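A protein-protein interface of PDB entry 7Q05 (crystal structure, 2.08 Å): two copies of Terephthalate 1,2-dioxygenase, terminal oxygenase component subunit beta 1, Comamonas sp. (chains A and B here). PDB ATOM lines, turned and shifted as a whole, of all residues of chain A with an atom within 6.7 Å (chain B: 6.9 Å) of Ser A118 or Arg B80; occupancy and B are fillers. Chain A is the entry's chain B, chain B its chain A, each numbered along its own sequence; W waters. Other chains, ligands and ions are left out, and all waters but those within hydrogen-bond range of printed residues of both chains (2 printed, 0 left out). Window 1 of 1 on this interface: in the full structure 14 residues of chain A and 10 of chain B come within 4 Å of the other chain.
The guanidinium group (NE) of Arg B80 lies close to the backbone carbonyl oxygen (O) of Gly A119.
The side-chain carboxylate (OD1) of Asp A142 lies within salt-bridge range of the guanidinium group (NH2) of Arg B80 (2.9 Å).
The side-chain carboxylate (OE1) of Glu A120 is in salt-bridge range of the side-chain amino group (NZ) of Lys B16, at 3.7 Å.
The backbone NH of Ile B82 is in hydrogen-bond range of the backbone carbonyl oxygen of Met B103 (2.8 Å).
The side-chain carboxylate (OD2) of Asp B19 lies within salt-bridge range of the guanidinium group (NH1) of Arg B80 (3.7 Å).
The backbone carbonyl oxygen (O) of Lys B16 lies within hydrogen-bond range of the side-chain hydroxyl (OG) of Ser B20 (2.9 Å).
The backbone carbonyl oxygen of Arg B78 sits at hydrogen-bond distance from the backbone NH of Ile B107 (2.9 Å).
N of Phe A102 lies within hydrogen-bond range of O of Gly A119.
The backbone NH (N) of Leu B105 lies within hydrogen-bond range of the backbone carbonyl oxygen (O) of Arg B80 (2.8 Å).
Arg B80 touches Pro A101 (NH1 to CB, 3.9 Å).
Met B103 touches Met A103 (CE to CE, 3.4 Å).
CD1 of Leu B105 touches SD of Met A103 (3.9 Å).
Val A115 touches Thr B113.
Arg B80 touches Ser A118.
CD1 of Leu B105 touches CB of Ser A118, at 3.7 Å.
Ser A118 touches Ile B107.
Ile B107 touches Asp A142.
Ser A143 touches Ile B107.
Of the printed residues of chain B, Ser A118 touches Arg B80, Leu B105 and Ile B107.
Printed residues of chain A within 4 Å of Arg B80: Pro A101 (3.9 Å), Ser A118 (3.997 Å), Gly A119 (3.5 Å) and Asp A142 (2.9 Å).
Of the printed residues of chain A, Lys B16 touches Glu A120 (3.7 Å).
Printed residues of chain B within 4 Å of Met A103: Met B103 and Leu B105.
Printed residues of chain A within 4 Å of Ile B107: Ser A118 (3.9 Å), Asp A142 (3.6 Å) and Ser A143 (3.9 Å).
Ala A117 touches none of the printed residues of chain B.
Val B104 touches none of the printed residues of chain A.
The nearest printed residue of chain A that does not touch Arg B80 is Glu A120 (4.1 Å).
The nearest printed residue of chain A that does not touch Leu B105 is Val A115 (4.2 Å).
Of the 15 printed residues of chain B, 6 touch a printed residue of chain A.
Along chain B the printed residues that touch a printed residue of chain A span positions 16 to 113.
Of the 17 printed residues of chain A, 8 touch a printed residue of chain B.
Printed residues of chain A that touch a printed residue of chain B: Pro A101, Met A103, Val A115, Ser A118, Gly A119, Glu A120, Asp A142 and Ser A143.
Hydrophobic or aromatic side chains of chain A that line the printed part of chain B: Pro A101, Met A103 and Val A115.
Met B103 touches its own counterpart, Met A103.
Positions printed for both chains: 103 and 104.
Of the 12 pairs that touch across the chains among the printed residues, 1 has its exchanged pair printed and touching as well.
Water W1 lies within hydrogen-bond range of the side-chain carboxylate of Glu A120 and the guanidinium group of Arg B80.
Water W2 lies within hydrogen-bond range of the side-chain hydroxyl (OG) of Ser A118 (2.7 Å) and the side-chain hydroxyl (OG1) of Thr B113 (2.8 Å).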
ATOM      1  N   VAL A  41     -25.151   5.931 -36.174  1.00  0.00           N
ATOM      2  CA  VAL A  41     -25.857   4.868 -35.396  1.00  0.00           C
ATOM      3  C   VAL A  41     -26.364   3.793 -36.350  1.00  0.00           C
ATOM      4  O   VAL A  41     -26.364   2.618 -35.922  1.00  0.00           O
ATOM      5  CB  VAL A  41     -26.999   5.444 -34.534  1.00  0.00           C
ATOM      6  CG1 VAL A  41     -26.419   6.216 -33.369  1.00  0.00           C
ATOM      7  CG2 VAL A  41     -27.932   6.310 -35.342  1.00  0.00           C
ATOM      8  N   THR A 100     -18.031   7.953 -24.258  1.00  0.00           N
ATOM      9  CA  THR A 100     -18.118   9.380 -23.899  1.00  0.00           C
ATOM     10  C   THR A 100     -19.122  10.069 -24.827  1.00  0.00           C
ATOM     11  O   THR A 100     -18.932  10.114 -26.030  1.00  0.00           O
ATOM     12  CB  THR A 100     -16.751  10.056 -23.959  1.00  0.00           C
ATOM     13  OG1 THR A 100     -15.868   9.361 -23.077  1.00  0.00           O
ATOM     14  CG2 THR A 100     -16.867  11.513 -23.578  1.00  0.00           C
ATOM     15  N   PRO A 101     -20.203  10.653 -24.301  1.00  0.00           N
ATOM     16  CA  PRO A 101     -21.094  11.449 -25.131  1.00  0.00           C
ATOM     17  C   PRO A 101     -20.406  12.727 -25.626  1.00  0.00           C
ATOM     18  O   PRO A 101     -19.628  13.315 -24.900  1.00  0.00           O
ATOM     19  CB  PRO A 101     -22.277  11.814 -24.210  1.00  0.00           C
ATOM     20  CG  PRO A 101     -22.150  10.877 -22.994  1.00  0.00           C
ATOM     21  CD  PRO A 101     -20.669  10.548 -22.897  1.00  0.00           C
ATOM     22  N   PHE A 102     -20.779  13.165 -26.821  1.00  0.00           N
ATOM     23  CA  PHE A 102     -20.231  14.421 -27.391  1.00  0.00           C
ATOM     24  C   PHE A 102     -21.306  15.162 -28.162  1.00  0.00           C
ATOM     25  O   PHE A 102     -22.212  14.570 -28.755  1.00  0.00           O
ATOM     26  CB  PHE A 102     -19.009  14.185 -28.299  1.00  0.00           C
ATOM     27  CG  PHE A 102     -19.273  13.467 -29.608  1.00  0.00           C
ATOM     28  CD1 PHE A 102     -19.740  14.160 -30.727  1.00  0.00           C
ATOM     29  CD2 PHE A 102     -18.973  12.124 -29.743  1.00  0.00           C
ATOM     30  CE1 PHE A 102     -19.960  13.507 -31.926  1.00  0.00           C
ATOM     31  CE2 PHE A 102     -19.197  11.462 -30.944  1.00  0.00           C
ATOM     32  CZ  PHE A 102     -19.692  12.155 -32.032  1.00  0.00           C
ATOM     33  N   MET A 103     -21.084  16.463 -28.229  1.00  0.00           N
ATOM     34  CA  MET A 103     -21.717  17.377 -29.173  1.00  0.00           C
ATOM     35  C   MET A 103     -20.591  18.241 -29.779  1.00  0.00           C
ATOM     36  O   MET A 103     -19.703  18.721 -29.030  1.00  0.00           O
ATOM     37  CB  MET A 103     -22.734  18.228 -28.422  1.00  0.00           C
ATOM     38  CG  MET A 103     -23.353  19.265 -29.287  1.00  0.00           C
ATOM     39  SD  MET A 103     -24.477  20.299 -28.334  1.00  0.00           S
ATOM     40  CE  MET A 103     -23.347  20.889 -27.102  1.00  0.00           C
ATOM     41  N   VAL A 104     -20.642  18.474 -31.095  1.00  0.00           N
ATOM     42  CA  VAL A 104     -19.725  19.413 -31.789  1.00  0.00           C
ATOM     43  C   VAL A 104     -20.544  20.531 -32.446  1.00  0.00           C
ATOM     44  O   VAL A 104     -21.441  20.224 -33.231  1.00  0.00           O
ATOM     45  CB  VAL A 104     -18.890  18.664 -32.818  1.00  0.00           C
ATOM     46  CG1 VAL A 104     -17.953  19.631 -33.540  1.00  0.00           C
ATOM     47  CG2 VAL A 104     -18.122  17.545 -32.159  1.00  0.00           C
ATOM     48  N   VAL A 115     -25.430  22.963 -34.557  1.00  0.00           N
ATOM     49  CA  VAL A 115     -25.042  21.648 -34.003  1.00  0.00           C
ATOM     50  C   VAL A 115     -24.620  20.825 -35.207  1.00  0.00           C
ATOM     51  O   VAL A 115     -25.481  20.533 -36.010  1.00  0.00           O
ATOM     52  CB  VAL A 115     -26.200  20.998 -33.235  1.00  0.00           C
ATOM     53  CG1 VAL A 115     -25.720  19.659 -32.673  1.00  0.00           C
ATOM     54  CG2 VAL A 115     -26.702  21.947 -32.175  1.00  0.00           C
ATOM     55  N   PHE A 116     -23.348  20.486 -35.304  1.00  0.00           N
ATOM     56  CA  PHE A 116     -22.790  19.843 -36.500  1.00  0.00           C
ATOM     57  C   PHE A 116     -22.806  18.331 -36.364  1.00  0.00           C
ATOM     58  O   PHE A 116     -23.014  17.633 -37.361  1.00  0.00           O
ATOM     59  CB  PHE A 116     -21.388  20.395 -36.746  1.00  0.00           C
ATOM     60  CG  PHE A 116     -20.639  19.738 -37.867  1.00  0.00           C
ATOM     61  CD1 PHE A 116     -20.956  20.027 -39.181  1.00  0.00           C
ATOM     62  CD2 PHE A 116     -19.569  18.905 -37.611  1.00  0.00           C
ATOM     63  CE1 PHE A 116     -20.246  19.413 -40.210  1.00  0.00           C
ATOM     64  CE2 PHE A 116     -18.849  18.306 -38.642  1.00  0.00           C
ATOM     65  CZ  PHE A 116     -19.222  18.532 -39.938  1.00  0.00           C
ATOM     66  N   ALA A 117     -22.518  17.828 -35.183  1.00  0.00           N
ATOM     67  CA  ALA A 117     -22.579  16.390 -34.878  1.00  0.00           C
ATOM     68  C   ALA A 117     -22.823  16.198 -33.379  1.00  0.00           C
ATOM     69  O   ALA A 117     -22.545  17.103 -32.549  1.00  0.00           O
ATOM     70  CB  ALA A 117     -21.306  15.753 -35.305  1.00  0.00           C
ATOM     71  N   SER A 118     -23.326  15.032 -33.044  1.00  0.00           N
ATOM     72  CA  SER A 118     -23.509  14.583 -31.650  1.00  0.00           C
ATOM     73  C   SER A 118     -23.389  13.061 -31.668  1.00  0.00           C
ATOM     74  O   SER A 118     -23.582  12.457 -32.744  1.00  0.00           O
ATOM     75  CB  SER A 118     -24.811  15.113 -31.067  1.00  0.00           C
ATOM     76  OG  SER A 118     -25.950  14.441 -31.610  1.00  0.00           O
ATOM     77  N   GLY A 119     -23.058  12.459 -30.532  1.00  0.00           N
ATOM     78  CA  GLY A 119     -23.084  11.006 -30.413  1.00  0.00           C
ATOM     79  C   GLY A 119     -22.225  10.538 -29.289  1.00  0.00           C
ATOM     80  O   GLY A 119     -22.243  11.156 -28.199  1.00  0.00           O
ATOM     81  N   GLU A 120     -21.508   9.446 -29.517  1.00  0.00           N
ATOM     82  CA  GLU A 120     -20.588   8.989 -28.463  1.00  0.00           C
ATOM     83  C   GLU A 120     -19.340   8.448 -29.115  1.00  0.00           C
ATOM     84  O   GLU A 120     -19.386   7.909 -30.229  1.00  0.00           O
ATOM     85  CB  GLU A 120     -21.188   7.990 -27.477  1.00  0.00           C
ATOM     86  CG  GLU A 120     -22.121   7.012 -28.059  1.00  0.00           C
ATOM     87  CD  GLU A 120     -22.589   5.939 -27.085  1.00  0.00           C
ATOM     88  OE1 GLU A 120     -22.405   6.087 -25.831  1.00  0.00           O
ATOM     89  OE2 GLU A 120     -23.119   4.962 -27.598  1.00  0.00           O
ATOM     90  N   VAL A 140     -19.357   7.616 -33.122  1.00  0.00           N
ATOM     91  CA  VAL A 140     -20.685   7.143 -33.592  1.00  0.00           C
ATOM     92  C   VAL A 140     -21.643   8.333 -33.540  1.00  0.00           C
ATOM     93  O   VAL A 140     -22.143   8.663 -32.431  1.00  0.00           O
ATOM     94  CB  VAL A 140     -21.207   5.940 -32.782  1.00  0.00           C
ATOM     95  CG1 VAL A 140     -22.508   5.389 -33.394  1.00  0.00           C
ATOM     96  CG2 VAL A 140     -20.207   4.814 -32.695  1.00  0.00           C
ATOM     97  N   CYS A 141     -21.913   8.941 -34.689  1.00  0.00           N
ATOM     98  CA  CYS A 141     -22.775  10.126 -34.806  1.00  0.00           C
ATOM     99  C   CYS A 141     -24.235   9.687 -34.692  1.00  0.00           C
ATOM    100  O   CYS A 141     -24.603   8.664 -35.278  1.00  0.00           O
ATOM    101  CB  CYS A 141     -22.493  10.931 -36.086  1.00  0.00           C
ATOM    102  SG  CYS A 141     -20.821  11.654 -36.102  1.00  0.00           S
ATOM    103  N   ASP A 142     -25.011  10.478 -33.954  1.00  0.00           N
ATOM    104  CA  ASP A 142     -26.472  10.289 -33.799  1.00  0.00           C
ATOM    105  C   ASP A 142     -27.152  10.458 -35.163  1.00  0.00           C
ATOM    106  O   ASP A 142     -28.192   9.795 -35.372  1.00  0.00           O
ATOM    107  CB  ASP A 142     -27.007  11.261 -32.749  1.00  0.00           C
ATOM    108  CG  ASP A 142     -26.482  10.986 -31.341  1.00  0.00           C
ATOM    109  OD1 ASP A 142     -26.296   9.771 -31.032  1.00  0.00           O
ATOM    110  OD2 ASP A 142     -26.236  11.985 -30.578  1.00  0.00           O
ATOM    111  N   SER A 143     -26.700  11.396 -35.994  1.00  0.00           N
ATOM    112  CA  SER A 143     -27.334  11.686 -37.325  1.00  0.00           C
ATOM    113  C   SER A 143     -26.575  10.977 -38.454  1.00  0.00           C
ATOM    114  O   SER A 143     -25.361  10.923 -38.414  1.00  0.00           O
ATOM    115  CB  SER A 143     -27.391  13.189 -37.571  1.00  0.00           C
ATOM    116  OG  SER A 143     -28.003  13.467 -38.837  1.00  0.00           O
ATOM    117  N   LEU A 154     -13.611  14.494 -35.699  1.00  0.00           N
ATOM    118  CA  LEU A 154     -14.442  14.656 -34.484  1.00  0.00           C
ATOM    119  C   LEU A 154     -13.653  14.149 -33.283  1.00  0.00           C
ATOM    120  O   LEU A 154     -12.828  13.227 -33.400  1.00  0.00           O
ATOM    121  CB  LEU A 154     -15.757  13.889 -34.654  1.00  0.00           C
ATOM    122  CG  LEU A 154     -16.648  14.352 -35.805  1.00  0.00           C
ATOM    123  CD1 LEU A 154     -17.937  13.535 -35.810  1.00  0.00           C
ATOM    124  CD2 LEU A 154     -16.947  15.830 -35.661  1.00  0.00           C
ATOM    125  OXT LEU A 154     -13.917  14.716 -32.224  1.00  0.00           O
ATOM    126  N   ALA B  15     -28.448   9.267 -18.138  1.00  0.00           N
ATOM    127  CA  ALA B  15     -28.390   9.813 -19.507  1.00  0.00           C
ATOM    128  C   ALA B  15     -28.090   8.668 -20.494  1.00  0.00           C
ATOM    129  O   ALA B  15     -28.750   8.597 -21.536  1.00  0.00           O
ATOM    130  CB  ALA B  15     -27.376  10.916 -19.587  1.00  0.00           C
ATOM    131  N   LYS B  16     -27.127   7.801 -20.172  1.00  0.00           N
ATOM    132  CA  LYS B  16     -26.761   6.705 -21.064  1.00  0.00           C
ATOM    133  C   LYS B  16     -27.972   5.801 -21.272  1.00  0.00           C
ATOM    134  O   LYS B  16     -28.192   5.359 -22.426  1.00  0.00           O
ATOM    135  CB  LYS B  16     -25.595   5.885 -20.532  1.00  0.00           C
ATOM    136  CG  LYS B  16     -24.974   4.949 -21.563  1.00  0.00           C
ATOM    137  CD  LYS B  16     -23.744   4.306 -20.974  1.00  0.00           C
ATOM    138  CE  LYS B  16     -23.173   3.186 -21.813  1.00  0.00           C
ATOM    139  NZ  LYS B  16     -23.149   3.619 -23.235  1.00  0.00           N
ATOM    140  N   ASP B  19     -30.608   7.634 -23.455  1.00  0.00           N
ATOM    141  CA  ASP B  19     -30.134   7.968 -24.810  1.00  0.00           C
ATOM    142  C   ASP B  19     -29.955   6.679 -25.621  1.00  0.00           C
ATOM    143  O   ASP B  19     -29.838   6.794 -26.820  1.00  0.00           O
ATOM    144  CB  ASP B  19     -28.868   8.793 -24.776  1.00  0.00           C
ATOM    145  CG  ASP B  19     -29.094  10.194 -24.261  1.00  0.00           C
ATOM    146  OD1 ASP B  19     -30.264  10.577 -24.072  1.00  0.00           O
ATOM    147  OD2 ASP B  19     -28.056  10.867 -24.009  1.00  0.00           O
ATOM    148  N   SER B  20     -29.888   5.516 -24.990  1.00  0.00           N
ATOM    149  CA  SER B  20     -29.534   4.247 -25.684  1.00  0.00           C
ATOM    150  C   SER B  20     -30.826   3.483 -25.976  1.00  0.00           C
ATOM    151  O   SER B  20     -30.772   2.357 -26.553  1.00  0.00           O
ATOM    152  CB  SER B  20     -28.601   3.412 -24.873  1.00  0.00           C
ATOM    153  OG  SER B  20     -29.305   2.971 -23.720  1.00  0.00           O
ATOM    154  N   ARG B  78     -34.095   9.974 -31.368  1.00  0.00           N
ATOM    155  CA  ARG B  78     -33.219   9.634 -30.242  1.00  0.00           C
ATOM    156  C   ARG B  78     -32.883  10.923 -29.533  1.00  0.00           C
ATOM    157  O   ARG B  78     -33.017  11.984 -30.136  1.00  0.00           O
ATOM    158  CB  ARG B  78     -31.932   8.944 -30.709  1.00  0.00           C
ATOM    159  CG  ARG B  78     -32.131   7.609 -31.414  1.00  0.00           C
ATOM    160  CD  ARG B  78     -32.596   6.465 -30.503  1.00  0.00           C
ATOM    161  NE  ARG B  78     -31.552   5.870 -29.647  1.00  0.00           N
ATOM    162  CZ  ARG B  78     -30.481   5.211 -30.094  1.00  0.00           C
ATOM    163  NH1 ARG B  78     -30.225   5.050 -31.394  1.00  0.00           N
ATOM    164  NH2 ARG B  78     -29.654   4.719 -29.202  1.00  0.00           N
ATOM    165  N   TYR B  79     -32.439  10.788 -28.295  1.00  0.00           N
ATOM    166  CA  TYR B  79     -31.986  11.910 -27.460  1.00  0.00           C
ATOM    167  C   TYR B  79     -30.476  11.832 -27.341  1.00  0.00           C
ATOM    168  O   TYR B  79     -29.892  10.724 -27.401  1.00  0.00           O
ATOM    169  CB  TYR B  79     -32.600  11.891 -26.067  1.00  0.00           C
ATOM    170  CG  TYR B  79     -34.037  12.295 -25.947  1.00  0.00           C
ATOM    171  CD1 TYR B  79     -34.734  12.900 -26.978  1.00  0.00           C
ATOM    172  CD2 TYR B  79     -34.701  12.042 -24.777  1.00  0.00           C
ATOM    173  CE1 TYR B  79     -36.053  13.292 -26.815  1.00  0.00           C
ATOM    174  CE2 TYR B  79     -36.016  12.432 -24.586  1.00  0.00           C
ATOM    175  CZ  TYR B  79     -36.696  13.082 -25.597  1.00  0.00           C
ATOM    176  OH  TYR B  79     -38.012  13.404 -25.378  1.00  0.00           O
ATOM    177  N   ARG B  80     -29.884  13.014 -27.193  1.00  0.00           N
ATOM    178  CA  ARG B  80     -28.507  13.166 -26.713  1.00  0.00           C
ATOM    179  C   ARG B  80     -28.536  14.154 -25.551  1.00  0.00           C
ATOM    180  O   ARG B  80     -28.783  15.370 -25.795  1.00  0.00           O
ATOM    181  CB  ARG B  80     -27.648  13.637 -27.897  1.00  0.00           C
ATOM    182  CG  ARG B  80     -26.186  13.844 -27.535  1.00  0.00           C
ATOM    183  CD  ARG B  80     -25.615  12.628 -26.809  1.00  0.00           C
ATOM    184  NE  ARG B  80     -25.656  11.480 -27.690  1.00  0.00           N
ATOM    185  CZ  ARG B  80     -25.461  10.237 -27.334  1.00  0.00           C
ATOM    186  NH1 ARG B  80     -25.188   9.913 -26.069  1.00  0.00           N
ATOM    187  NH2 ARG B  80     -25.487   9.303 -28.268  1.00  0.00           N
ATOM    188  N   HIS B  81     -28.377  13.653 -24.349  1.00  0.00           N
ATOM    189  CA  HIS B  81     -28.287  14.435 -23.088  1.00  0.00           C
ATOM    190  C   HIS B  81     -26.856  14.953 -22.941  1.00  0.00           C
ATOM    191  O   HIS B  81     -25.930  14.111 -23.017  1.00  0.00           O
ATOM    192  CB  HIS B  81     -28.565  13.527 -21.892  1.00  0.00           C
ATOM    193  CG  HIS B  81     -29.997  13.258 -21.671  1.00  0.00           C
ATOM    194  ND1 HIS B  81     -30.691  12.423 -22.495  1.00  0.00           N
ATOM    195  CD2 HIS B  81     -30.857  13.689 -20.704  1.00  0.00           C
ATOM    196  CE1 HIS B  81     -31.945  12.353 -22.067  1.00  0.00           C
ATOM    197  NE2 HIS B  81     -32.073  13.132 -20.978  1.00  0.00           N
ATOM    198  N   ILE B  82     -26.699  16.260 -22.776  1.00  0.00           N
ATOM    199  CA  ILE B  82     -25.444  16.887 -22.302  1.00  0.00           C
ATOM    200  C   ILE B  82     -25.756  17.545 -20.965  1.00  0.00           C
ATOM    201  O   ILE B  82     -26.644  18.391 -20.925  1.00  0.00           O
ATOM    202  CB  ILE B  82     -24.923  17.901 -23.332  1.00  0.00           C
ATOM    203  CG1 ILE B  82     -24.794  17.306 -24.727  1.00  0.00           C
ATOM    204  CG2 ILE B  82     -23.620  18.481 -22.826  1.00  0.00           C
ATOM    205  CD1 ILE B  82     -23.687  16.266 -24.835  1.00  0.00           C
ATOM    206  N   MET B 103     -29.139  19.759 -21.129  1.00  0.00           N
ATOM    207  CA  MET B 103     -29.594  20.049 -22.496  1.00  0.00           C
ATOM    208  C   MET B 103     -29.895  18.689 -23.152  1.00  0.00           C
ATOM    209  O   MET B 103     -29.028  17.788 -23.068  1.00  0.00           O
ATOM    210  CB  MET B 103     -28.512  20.815 -23.258  1.00  0.00           C
ATOM    211  CG  MET B 103     -28.843  20.987 -24.756  1.00  0.00           C
ATOM    212  SD  MET B 103     -27.434  21.853 -25.591  1.00  0.00           S
ATOM    213  CE  MET B 103     -26.088  20.775 -25.119  1.00  0.00           C
ATOM    214  N   VAL B 104     -31.006  18.587 -23.884  1.00  0.00           N
ATOM    215  CA  VAL B 104     -31.346  17.380 -24.675  1.00  0.00           C
ATOM    216  C   VAL B 104     -31.485  17.723 -26.141  1.00  0.00           C
ATOM    217  O   VAL B 104     -32.288  18.596 -26.492  1.00  0.00           O
ATOM    218  CB  VAL B 104     -32.636  16.744 -24.139  1.00  0.00           C
ATOM    219  CG1 VAL B 104     -32.970  15.509 -24.951  1.00  0.00           C
ATOM    220  CG2 VAL B 104     -32.435  16.386 -22.668  1.00  0.00           C
ATOM    221  N   LEU B 105     -30.635  17.119 -26.956  1.00  0.00           N
ATOM    222  CA  LEU B 105     -30.792  17.164 -28.415  1.00  0.00           C
ATOM    223  C   LEU B 105     -31.787  16.085 -28.803  1.00  0.00           C
ATOM    224  O   LEU B 105     -31.725  15.016 -28.237  1.00  0.00           O
ATOM    225  CB  LEU B 105     -29.454  16.983 -29.131  1.00  0.00           C
ATOM    226  CG  LEU B 105     -28.337  17.925 -28.671  1.00  0.00           C
ATOM    227  CD1 LEU B 105     -27.034  17.520 -29.319  1.00  0.00           C
ATOM    228  CD2 LEU B 105     -28.691  19.383 -28.989  1.00  0.00           C
ATOM    229  N   ARG B 106     -32.646  16.392 -29.760  1.00  0.00           N
ATOM    230  CA  ARG B 106     -33.446  15.384 -30.458  1.00  0.00           C
ATOM    231  C   ARG B 106     -32.856  15.208 -31.852  1.00  0.00           C
ATOM    232  O   ARG B 106     -32.701  16.204 -32.547  1.00  0.00           O
ATOM    233  CB  ARG B 106     -34.916  15.790 -30.520  1.00  0.00           C
ATOM    234  CG  ARG B 106     -35.768  14.749 -31.228  1.00  0.00           C
ATOM    235  CD  ARG B 106     -37.198  15.167 -31.354  1.00  0.00           C
ATOM    236  NE  ARG B 106     -37.280  16.290 -32.280  1.00  0.00           N
ATOM    237  CZ  ARG B 106     -38.309  17.123 -32.376  1.00  0.00           C
ATOM    238  NH1 ARG B 106     -38.265  18.110 -33.240  1.00  0.00           N
ATOM    239  NH2 ARG B 106     -39.403  16.942 -31.653  1.00  0.00           N
ATOM    240  N   ILE B 107     -32.565  13.955 -32.209  1.00  0.00           N
ATOM    241  CA  ILE B 107     -32.117  13.565 -33.559  1.00  0.00           C
ATOM    242  C   ILE B 107     -33.194  12.657 -34.160  1.00  0.00           C
ATOM    243  O   ILE B 107     -33.320  11.536 -33.709  1.00  0.00           O
ATOM    244  CB  ILE B 107     -30.728  12.916 -33.538  1.00  0.00           C
ATOM    245  CG1 ILE B 107     -29.737  13.731 -32.705  1.00  0.00           C
ATOM    246  CG2 ILE B 107     -30.250  12.695 -34.955  1.00  0.00           C
ATOM    247  CD1 ILE B 107     -29.657  13.338 -31.270  1.00  0.00           C
ATOM    248  N   THR B 113     -31.138  17.495 -36.243  1.00  0.00           N
ATOM    249  CA  THR B 113     -30.720  17.658 -34.839  1.00  0.00           C
ATOM    250  C   THR B 113     -31.223  19.002 -34.362  1.00  0.00           C
ATOM    251  O   THR B 113     -30.908  19.950 -35.013  1.00  0.00           O
ATOM    252  CB  THR B 113     -29.213  17.584 -34.682  1.00  0.00           C
ATOM    253  OG1 THR B 113     -28.848  16.305 -35.181  1.00  0.00           O
ATOM    254  CG2 THR B 113     -28.762  17.742 -33.246  1.00  0.00           C
HETATM  255  O   HOH W   1     -24.338   7.466 -24.493  1.00  0.00           O
HETATM  256  O   HOH W   2     -26.584  14.926 -34.231  1.00  0.00           O
